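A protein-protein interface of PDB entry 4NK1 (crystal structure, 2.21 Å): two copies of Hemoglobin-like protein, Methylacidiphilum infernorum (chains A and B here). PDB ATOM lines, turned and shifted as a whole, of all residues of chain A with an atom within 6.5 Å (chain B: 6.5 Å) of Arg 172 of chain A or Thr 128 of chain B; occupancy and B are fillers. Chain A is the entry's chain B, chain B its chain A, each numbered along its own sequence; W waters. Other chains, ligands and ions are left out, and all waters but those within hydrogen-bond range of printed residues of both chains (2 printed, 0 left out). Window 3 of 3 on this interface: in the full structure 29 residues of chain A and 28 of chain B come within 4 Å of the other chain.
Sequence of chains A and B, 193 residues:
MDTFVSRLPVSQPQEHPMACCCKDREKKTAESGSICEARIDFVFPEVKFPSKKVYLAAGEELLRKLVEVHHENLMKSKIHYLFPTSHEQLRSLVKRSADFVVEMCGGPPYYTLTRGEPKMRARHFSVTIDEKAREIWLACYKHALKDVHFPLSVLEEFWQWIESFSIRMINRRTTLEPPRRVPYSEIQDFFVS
Of the 13 printed residues of chain B, 6 touch a printed residue of chain A. Hydrophobic or aromatic side chains of chain B within 4 Å of the printed part of chain A: Phe 125. Of the 11 printed residues of chain A, 6 touch a printed residue of chain B. Printed residues of chain A that touch a printed residue of chain B: Thr 128, Asn 171, Arg 172, Arg 173, Thr 174 and Thr 175.
Glu 131 of chain A touches none of the printed residues of chain B. Printed residues of chain B within 4 Å of Asn 171 of chain A: Asn 171 (3.5 Å), Arg 172 (3.2 Å) and Arg 173 (2.8 Å). Arg 172 of chain A touches just these residues of chain B: Phe 125 (2.7 Å), Val 127 (3.6 Å), Thr 128 (3.2 Å) and Asn 171 (3.2 Å). Printed residues of chain B within 4 Å of Arg 173 of chain A: Phe 125 and Asn 171. Printed residues of chain A within 4 Å of Val 127 of chain B: Arg 172. Of chain A, only Arg 172 (3.2 Å) comes within 4 Å of Thr 128 of chain B. Of the printed residues of chain A, Asn 171 of chain B touches Asn 171, Arg 172 and Arg 173. The nearest residue of chain B that does not touch Arg 172 of chain A is Arg 172 of chain B (4.3 Å).
The backbone carbonyl oxygen (O) of Phe 125 of chain B sits at hydrogen-bond distance from the guanidinium group (NH2) of Arg 172 of chain A (2.7 Å). NH2 of Arg 172 of chain A lies within hydrogen-bond range of OG1 of Thr 128 of chain B. The backbone carbonyl oxygen (O) of Asn 171 of chain B lies within hydrogen-bond range of the backbone NH (N) of Arg 173 of chain A (2.9 Å). The side-chain hydroxyl of Thr 128 of chain A sits at hydrogen-bond distance from the guanidinium group of Arg 172 of chain B. The backbone NH (N) of Arg 173 of chain B sits at hydrogen-bond distance from the backbone carbonyl oxygen (O) of Asn 171 of chain A (2.8 Å). The backbone carbonyl oxygen of Asn 171 of chain A sits close to the backbone carbonyl oxygen of Asn 171 of chain B, 3.5 Å away.
Thr 128 of chain A touches Arg 172 of chain B, and with the chains exchanged Arg 172 of chain A touches Thr 128 of chain B. Asn 171 of chain B touches its own counterpart, Asn 171 of chain A. Asn 171 of chain A touches Arg 172 of chain B, and with the chains exchanged Arg 172 of chain A touches Asn 171 of chain B. Asn 171 of chain A touches Arg 173 of chain B, and with the chains exchanged Arg 173 of chain A touches Asn 171 of chain B. Positions printed for both chains: 128, 129, 130, 171, 172 and 173.
Water W2 lies within hydrogen-bond range of OG1 of Thr 128 of chain A and NE of Arg 172 of chain B. Water W1 bridges O of Asn 171 of chain B (3.0 Å) and O of Asn 171 of chain A (3.1 Å).
Among the printed residues, pairs that only touch across the chains: Asn 171 of chain A with Arg 172 of chain B, Arg 172 of chain A with Val 127 of chain B, Arg 172 of chain A with Asn 171 of chain B, Arg 173 of chain A with Phe 125 of chain B, Thr 174 of chain A with Phe 125 of chain B and Thr 175 of chain A with Phe 125 of chain B.
N of Arg 172 of chain B is in hydrogen-bond range of O of Ile 129 of chain B. N of Ile 129 of chain A sits at hydrogen-bond distance from OD1 of Asn 171 of chain A, 2.8 Å away. The backbone NH (N) of Arg 172 of chain A lies within hydrogen-bond range of the backbone carbonyl oxygen (O) of Ile 129 of chain A. OE2 of Glu 131 of chain A is in salt-bridge range of NH1 of Arg 173 of chain A. The side-chain hydroxyl (OG1) of Thr 174 of chain A is in hydrogen-bond range of the side-chain carboxylate (OE1) of Glu 131 of chain A (2.6 Å). The guanidinium group of Arg 173 of chain A is in hydrogen-bond range of the backbone carbonyl oxygen of Thr 175 of chain A, at 3.2 Å.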
ATOM      1  N   THR A 128      22.625  -4.283  -9.987  1.00  0.00           N
ATOM      2  CA  THR A 128      22.191  -2.886 -10.100  1.00  0.00           C
ATOM      3  C   THR A 128      22.330  -2.402 -11.531  1.00  0.00           C
ATOM      4  O   THR A 128      23.447  -2.338 -12.080  1.00  0.00           O
ATOM      5  CB  THR A 128      22.951  -1.967  -9.136  1.00  0.00           C
ATOM      6  OG1 THR A 128      22.691  -2.408  -7.801  1.00  0.00           O
ATOM      7  CG2 THR A 128      22.499  -0.490  -9.276  1.00  0.00           C
ATOM      8  N   ILE A 129      21.192  -2.082 -12.145  1.00  0.00           N
ATOM      9  CA  ILE A 129      21.190  -1.673 -13.547  1.00  0.00           C
ATOM     10  C   ILE A 129      20.541  -0.313 -13.675  1.00  0.00           C
ATOM     11  O   ILE A 129      19.307  -0.178 -13.545  1.00  0.00           O
ATOM     12  CB  ILE A 129      20.440  -2.683 -14.450  1.00  0.00           C
ATOM     13  CG1 ILE A 129      21.062  -4.079 -14.332  1.00  0.00           C
ATOM     14  CG2 ILE A 129      20.448  -2.216 -15.912  1.00  0.00           C
ATOM     15  CD1 ILE A 129      20.419  -5.108 -15.226  1.00  0.00           C
ATOM     16  N   ASP A 130      21.361   0.707 -13.919  1.00  0.00           N
ATOM     17  CA  ASP A 130      20.787   2.035 -14.106  1.00  0.00           C
ATOM     18  C   ASP A 130      20.745   2.357 -15.593  1.00  0.00           C
ATOM     19  O   ASP A 130      21.072   1.499 -16.426  1.00  0.00           O
ATOM     20  CB  ASP A 130      21.525   3.109 -13.300  1.00  0.00           C
ATOM     21  CG  ASP A 130      22.997   3.263 -13.703  1.00  0.00           C
ATOM     22  OD1 ASP A 130      23.436   2.700 -14.744  1.00  0.00           O
ATOM     23  OD2 ASP A 130      23.718   3.977 -12.966  1.00  0.00           O
ATOM     24  N   GLU A 131      20.344   3.576 -15.930  1.00  0.00           N
ATOM     25  CA  GLU A 131      20.163   3.937 -17.325  1.00  0.00           C
ATOM     26  C   GLU A 131      21.469   3.859 -18.133  1.00  0.00           C
ATOM     27  O   GLU A 131      21.468   3.360 -19.262  1.00  0.00           O
ATOM     28  CB  GLU A 131      19.504   5.314 -17.420  1.00  0.00           C
ATOM     29  CG  GLU A 131      18.236   5.441 -16.559  1.00  0.00           C
ATOM     30  CD  GLU A 131      18.502   6.053 -15.172  1.00  0.00           C
ATOM     31  OE1 GLU A 131      19.676   6.138 -14.743  1.00  0.00           O
ATOM     32  OE2 GLU A 131      17.527   6.468 -14.509  1.00  0.00           O
ATOM     33  N   MET A 169      14.986  -4.046 -17.821  1.00  0.00           N
ATOM     34  CA  MET A 169      15.929  -4.577 -16.854  1.00  0.00           C
ATOM     35  C   MET A 169      16.392  -3.478 -15.897  1.00  0.00           C
ATOM     36  O   MET A 169      16.971  -3.771 -14.855  1.00  0.00           O
ATOM     37  CB  MET A 169      17.128  -5.217 -17.569  1.00  0.00           C
ATOM     38  CG  MET A 169      16.738  -6.194 -18.678  1.00  0.00           C
ATOM     39  SD  MET A 169      15.619  -7.508 -18.134  1.00  0.00           S
ATOM     40  CE  MET A 169      14.676  -7.723 -19.645  1.00  0.00           C
ATOM     41  N   ILE A 170      16.121  -2.217 -16.241  1.00  0.00           N
ATOM     42  CA  ILE A 170      16.563  -1.076 -15.437  1.00  0.00           C
ATOM     43  C   ILE A 170      15.883  -1.096 -14.070  1.00  0.00           C
ATOM     44  O   ILE A 170      14.647  -1.033 -13.971  1.00  0.00           O
ATOM     45  CB  ILE A 170      16.239   0.279 -16.116  1.00  0.00           C
ATOM     46  CG1 ILE A 170      17.068   0.474 -17.383  1.00  0.00           C
ATOM     47  CG2 ILE A 170      16.517   1.430 -15.168  1.00  0.00           C
ATOM     48  CD1 ILE A 170      16.538   1.597 -18.260  1.00  0.00           C
ATOM     49  N   ASN A 171      16.684  -1.176 -13.014  1.00  0.00           N
ATOM     50  CA  ASN A 171      16.133  -1.268 -11.665  1.00  0.00           C
ATOM     51  C   ASN A 171      16.641  -0.156 -10.735  1.00  0.00           C
ATOM     52  O   ASN A 171      16.220  -0.064  -9.578  1.00  0.00           O
ATOM     53  CB  ASN A 171      16.349  -2.677 -11.074  1.00  0.00           C
ATOM     54  CG  ASN A 171      17.828  -3.103 -11.066  1.00  0.00           C
ATOM     55  OD1 ASN A 171      18.720  -2.288 -10.818  1.00  0.00           O
ATOM     56  ND2 ASN A 171      18.082  -4.389 -11.328  1.00  0.00           N
ATOM     57  N   ARG A 172      17.539   0.687 -11.248  1.00  0.00           N
ATOM     58  CA  ARG A 172      18.010   1.845 -10.500  1.00  0.00           C
ATOM     59  C   ARG A 172      17.828   3.092 -11.356  1.00  0.00           C
ATOM     60  O   ARG A 172      18.383   3.192 -12.458  1.00  0.00           O
ATOM     61  CB  ARG A 172      19.480   1.681 -10.093  1.00  0.00           C
ATOM     62  CG  ARG A 172      20.108   2.935  -9.462  1.00  0.00           C
ATOM     63  CD  ARG A 172      19.504   3.243  -8.083  1.00  0.00           C
ATOM     64  NE  ARG A 172      20.429   3.955  -7.183  1.00  0.00           N
ATOM     65  CZ  ARG A 172      20.466   5.275  -7.003  1.00  0.00           C
ATOM     66  NH1 ARG A 172      19.652   6.069  -7.681  1.00  0.00           N
ATOM     67  NH2 ARG A 172      21.316   5.810  -6.129  1.00  0.00           N
ATOM     68  N   ARG A 173      17.032   4.033 -10.859  1.00  0.00           N
ATOM     69  CA  ARG A 173      16.825   5.290 -11.568  1.00  0.00           C
ATOM     70  C   ARG A 173      17.727   6.359 -10.995  1.00  0.00           C
ATOM     71  O   ARG A 173      18.009   6.383  -9.790  1.00  0.00           O
ATOM     72  CB  ARG A 173      15.355   5.724 -11.473  1.00  0.00           C
ATOM     73  CG  ARG A 173      14.462   4.807 -12.293  1.00  0.00           C
ATOM     74  CD  ARG A 173      14.634   5.087 -13.773  1.00  0.00           C
ATOM     75  NE  ARG A 173      13.725   6.156 -14.197  1.00  0.00           N
ATOM     76  CZ  ARG A 173      14.004   7.035 -15.153  1.00  0.00           C
ATOM     77  NH1 ARG A 173      15.171   6.980 -15.786  1.00  0.00           N
ATOM     78  NH2 ARG A 173      13.123   7.974 -15.469  1.00  0.00           N
ATOM     79  N   THR A 174      18.209   7.237 -11.866  1.00  0.00           N
ATOM     80  CA  THR A 174      19.137   8.278 -11.444  1.00  0.00           C
ATOM     81  C   THR A 174      18.765   9.591 -12.111  1.00  0.00           C
ATOM     82  O   THR A 174      19.449  10.596 -11.943  1.00  0.00           O
ATOM     83  CB  THR A 174      20.587   7.952 -11.830  1.00  0.00           C
ATOM     84  OG1 THR A 174      20.723   8.025 -13.255  1.00  0.00           O
ATOM     85  CG2 THR A 174      20.971   6.563 -11.354  1.00  0.00           C
ATOM     86  N   THR A 175      17.673   9.577 -12.868  1.00  0.00           N
ATOM     87  CA  THR A 175      17.219  10.790 -13.515  1.00  0.00           C
ATOM     88  C   THR A 175      15.712  10.775 -13.669  1.00  0.00           C
ATOM     89  O   THR A 175      15.081   9.716 -13.647  1.00  0.00           O
ATOM     90  CB  THR A 175      17.884  10.984 -14.905  1.00  0.00           C
ATOM     91  OG1 THR A 175      17.356  12.161 -15.533  1.00  0.00           O
ATOM     92  CG2 THR A 175      17.620   9.775 -15.794  1.00  0.00           C
ATOM     93  N   TYR B  81      22.968   2.990   7.881  1.00  0.00           N
ATOM     94  CA  TYR B  81      24.178   3.077   7.049  1.00  0.00           C
ATOM     95  C   TYR B  81      24.068   4.124   5.929  1.00  0.00           C
ATOM     96  O   TYR B  81      25.087   4.568   5.385  1.00  0.00           O
ATOM     97  CB  TYR B  81      24.569   1.688   6.494  1.00  0.00           C
ATOM     98  CG  TYR B  81      23.670   1.186   5.380  1.00  0.00           C
ATOM     99  CD1 TYR B  81      22.453   0.575   5.661  1.00  0.00           C
ATOM    100  CD2 TYR B  81      24.041   1.318   4.048  1.00  0.00           C
ATOM    101  CE1 TYR B  81      21.630   0.115   4.646  1.00  0.00           C
ATOM    102  CE2 TYR B  81      23.217   0.863   3.029  1.00  0.00           C
ATOM    103  CZ  TYR B  81      22.014   0.266   3.339  1.00  0.00           C
ATOM    104  OH  TYR B  81      21.189  -0.193   2.334  1.00  0.00           O
ATOM    105  N   LEU B  82      22.844   4.539   5.603  1.00  0.00           N
ATOM    106  CA  LEU B  82      22.642   5.534   4.549  1.00  0.00           C
ATOM    107  C   LEU B  82      22.890   6.965   5.011  1.00  0.00           C
ATOM    108  O   LEU B  82      22.903   7.887   4.196  1.00  0.00           O
ATOM    109  CB  LEU B  82      21.228   5.440   3.975  1.00  0.00           C
ATOM    110  CG  LEU B  82      20.889   4.124   3.287  1.00  0.00           C
ATOM    111  CD1 LEU B  82      19.403   4.055   2.961  1.00  0.00           C
ATOM    112  CD2 LEU B  82      21.731   3.969   2.028  1.00  0.00           C
ATOM    113  N   HIS B 124      16.958  12.782  -4.008  1.00  0.00           N
ATOM    114  CA  HIS B 124      17.208  11.459  -3.421  1.00  0.00           C
ATOM    115  C   HIS B 124      17.852  10.428  -4.334  1.00  0.00           C
ATOM    116  O   HIS B 124      18.197   9.332  -3.875  1.00  0.00           O
ATOM    117  CB  HIS B 124      15.924  10.886  -2.821  1.00  0.00           C
ATOM    118  CG  HIS B 124      15.508  11.586  -1.571  1.00  0.00           C
ATOM    119  ND1 HIS B 124      14.857  12.799  -1.586  1.00  0.00           N
ATOM    120  CD2 HIS B 124      15.706  11.276  -0.267  1.00  0.00           C
ATOM    121  CE1 HIS B 124      14.645  13.195  -0.343  1.00  0.00           C
ATOM    122  NE2 HIS B 124      15.148  12.288   0.470  1.00  0.00           N
ATOM    123  N   PHE B 125      17.996  10.750  -5.614  1.00  0.00           N
ATOM    124  CA  PHE B 125      18.725   9.866  -6.527  1.00  0.00           C
ATOM    125  C   PHE B 125      20.128   9.519  -5.974  1.00  0.00           C
ATOM    126  O   PHE B 125      20.662   8.450  -6.250  1.00  0.00           O
ATOM    127  CB  PHE B 125      18.848  10.513  -7.913  1.00  0.00           C
ATOM    128  CG  PHE B 125      17.571  10.471  -8.726  1.00  0.00           C
ATOM    129  CD1 PHE B 125      16.701   9.396  -8.621  1.00  0.00           C
ATOM    130  CD2 PHE B 125      17.248  11.500  -9.606  1.00  0.00           C
ATOM    131  CE1 PHE B 125      15.516   9.343  -9.376  1.00  0.00           C
ATOM    132  CE2 PHE B 125      16.078  11.457 -10.348  1.00  0.00           C
ATOM    133  CZ  PHE B 125      15.211  10.375 -10.235  1.00  0.00           C
ATOM    134  N   SER B 126      20.688  10.421  -5.167  1.00  0.00           N
ATOM    135  CA  SER B 126      22.026  10.269  -4.588  1.00  0.00           C
ATOM    136  C   SER B 126      22.072   9.334  -3.386  1.00  0.00           C
ATOM    137  O   SER B 126      23.136   9.154  -2.773  1.00  0.00           O
ATOM    138  CB  SER B 126      22.551  11.637  -4.137  1.00  0.00           C
ATOM    139  OG  SER B 126      22.411  12.586  -5.177  1.00  0.00           O
ATOM    140  N   VAL B 127      20.918   8.785  -3.019  1.00  0.00           N
ATOM    141  CA  VAL B 127      20.849   7.754  -1.995  1.00  0.00           C
ATOM    142  C   VAL B 127      20.176   6.573  -2.655  1.00  0.00           C
ATOM    143  O   VAL B 127      19.218   6.744  -3.413  1.00  0.00           O
ATOM    144  CB  VAL B 127      19.984   8.211  -0.803  1.00  0.00           C
ATOM    145  CG1 VAL B 127      20.060   7.211   0.326  1.00  0.00           C
ATOM    146  CG2 VAL B 127      20.444   9.563  -0.315  1.00  0.00           C
ATOM    147  N   THR B 128      20.663   5.371  -2.391  1.00  0.00           N
ATOM    148  CA  THR B 128      20.004   4.204  -2.957  1.00  0.00           C
ATOM    149  C   THR B 128      18.845   3.784  -2.060  1.00  0.00           C
ATOM    150  O   THR B 128      19.037   3.408  -0.892  1.00  0.00           O
ATOM    151  CB  THR B 128      20.982   3.051  -3.164  1.00  0.00           C
ATOM    152  OG1 THR B 128      21.991   3.464  -4.098  1.00  0.00           O
ATOM    153  CG2 THR B 128      20.244   1.821  -3.703  1.00  0.00           C
ATOM    154  N   ILE B 129      17.637   3.863  -2.604  1.00  0.00           N
ATOM    155  CA  ILE B 129      16.442   3.654  -1.799  1.00  0.00           C
ATOM    156  C   ILE B 129      15.562   2.590  -2.418  1.00  0.00           C
ATOM    157  O   ILE B 129      14.928   2.831  -3.462  1.00  0.00           O
ATOM    158  CB  ILE B 129      15.615   4.951  -1.671  1.00  0.00           C
ATOM    159  CG1 ILE B 129      16.475   6.079  -1.081  1.00  0.00           C
ATOM    160  CG2 ILE B 129      14.338   4.704  -0.827  1.00  0.00           C
ATOM    161  CD1 ILE B 129      15.769   7.404  -0.989  1.00  0.00           C
ATOM    162  N   ASP B 130      15.526   1.410  -1.798  1.00  0.00           N
ATOM    163  CA  ASP B 130      14.619   0.371  -2.281  1.00  0.00           C
ATOM    164  C   ASP B 130      13.313   0.390  -1.490  1.00  0.00           C
ATOM    165  O   ASP B 130      13.097   1.288  -0.670  1.00  0.00           O
ATOM    166  CB  ASP B 130      15.271  -1.014  -2.276  1.00  0.00           C
ATOM    167  CG  ASP B 130      15.724  -1.452  -0.900  1.00  0.00           C
ATOM    168  OD1 ASP B 130      15.360  -0.797   0.105  1.00  0.00           O
ATOM    169  OD2 ASP B 130      16.447  -2.477  -0.818  1.00  0.00           O
ATOM    170  N   ALA B 133      13.606   0.140   2.358  1.00  0.00           N
ATOM    171  CA  ALA B 133      14.133   1.372   2.928  1.00  0.00           C
ATOM    172  C   ALA B 133      13.004   2.371   3.180  1.00  0.00           C
ATOM    173  O   ALA B 133      12.988   3.052   4.205  1.00  0.00           O
ATOM    174  CB  ALA B 133      15.190   1.967   2.021  1.00  0.00           C
ATOM    175  N   ASN B 171      14.116   4.563  -5.647  1.00  0.00           N
ATOM    176  CA  ASN B 171      14.823   4.611  -6.918  1.00  0.00           C
ATOM    177  C   ASN B 171      15.513   3.291  -7.248  1.00  0.00           C
ATOM    178  O   ASN B 171      16.215   3.175  -8.263  1.00  0.00           O
ATOM    179  CB  ASN B 171      15.795   5.796  -6.948  1.00  0.00           C
ATOM    180  CG  ASN B 171      16.768   5.780  -5.787  1.00  0.00           C
ATOM    181  OD1 ASN B 171      17.260   4.715  -5.394  1.00  0.00           O
ATOM    182  ND2 ASN B 171      17.046   6.961  -5.219  1.00  0.00           N
ATOM    183  N   ARG B 172      15.289   2.289  -6.397  1.00  0.00           N
ATOM    184  CA  ARG B 172      15.869   0.966  -6.608  1.00  0.00           C
ATOM    185  C   ARG B 172      14.806  -0.115  -6.427  1.00  0.00           C
ATOM    186  O   ARG B 172      14.320  -0.337  -5.309  1.00  0.00           O
ATOM    187  CB  ARG B 172      17.053   0.735  -5.654  1.00  0.00           C
ATOM    188  CG  ARG B 172      17.658  -0.685  -5.704  1.00  0.00           C
ATOM    189  CD  ARG B 172      18.158  -1.046  -7.096  1.00  0.00           C
ATOM    190  NE  ARG B 172      19.240  -2.036  -7.087  1.00  0.00           N
ATOM    191  CZ  ARG B 172      19.087  -3.319  -7.397  1.00  0.00           C
ATOM    192  NH1 ARG B 172      17.891  -3.790  -7.730  1.00  0.00           N
ATOM    193  NH2 ARG B 172      20.126  -4.135  -7.371  1.00  0.00           N
ATOM    194  N   ARG B 173      14.440  -0.779  -7.526  1.00  0.00           N
ATOM    195  CA  ARG B 173      13.404  -1.803  -7.482  1.00  0.00           C
ATOM    196  C   ARG B 173      14.007  -3.186  -7.304  1.00  0.00           C
ATOM    197  O   ARG B 173      15.021  -3.527  -7.933  1.00  0.00           O
ATOM    198  CB  ARG B 173      12.547  -1.764  -8.749  1.00  0.00           C
ATOM    199  CG  ARG B 173      11.728  -0.497  -8.863  1.00  0.00           C
ATOM    200  CD  ARG B 173      10.534  -0.563  -7.940  1.00  0.00           C
ATOM    201  NE  ARG B 173       9.400  -1.203  -8.591  1.00  0.00           N
ATOM    202  CZ  ARG B 173       8.500  -1.960  -7.965  1.00  0.00           C
ATOM    203  NH1 ARG B 173       8.603  -2.182  -6.658  1.00  0.00           N
ATOM    204  NH2 ARG B 173       7.495  -2.502  -8.648  1.00  0.00           N
HETATM  205  O   HOH W   1      14.020   2.113 -10.056  1.00  0.00           O
HETATM  206  O   HOH W   2      21.732  -1.050  -5.863  1.00  0.00           O
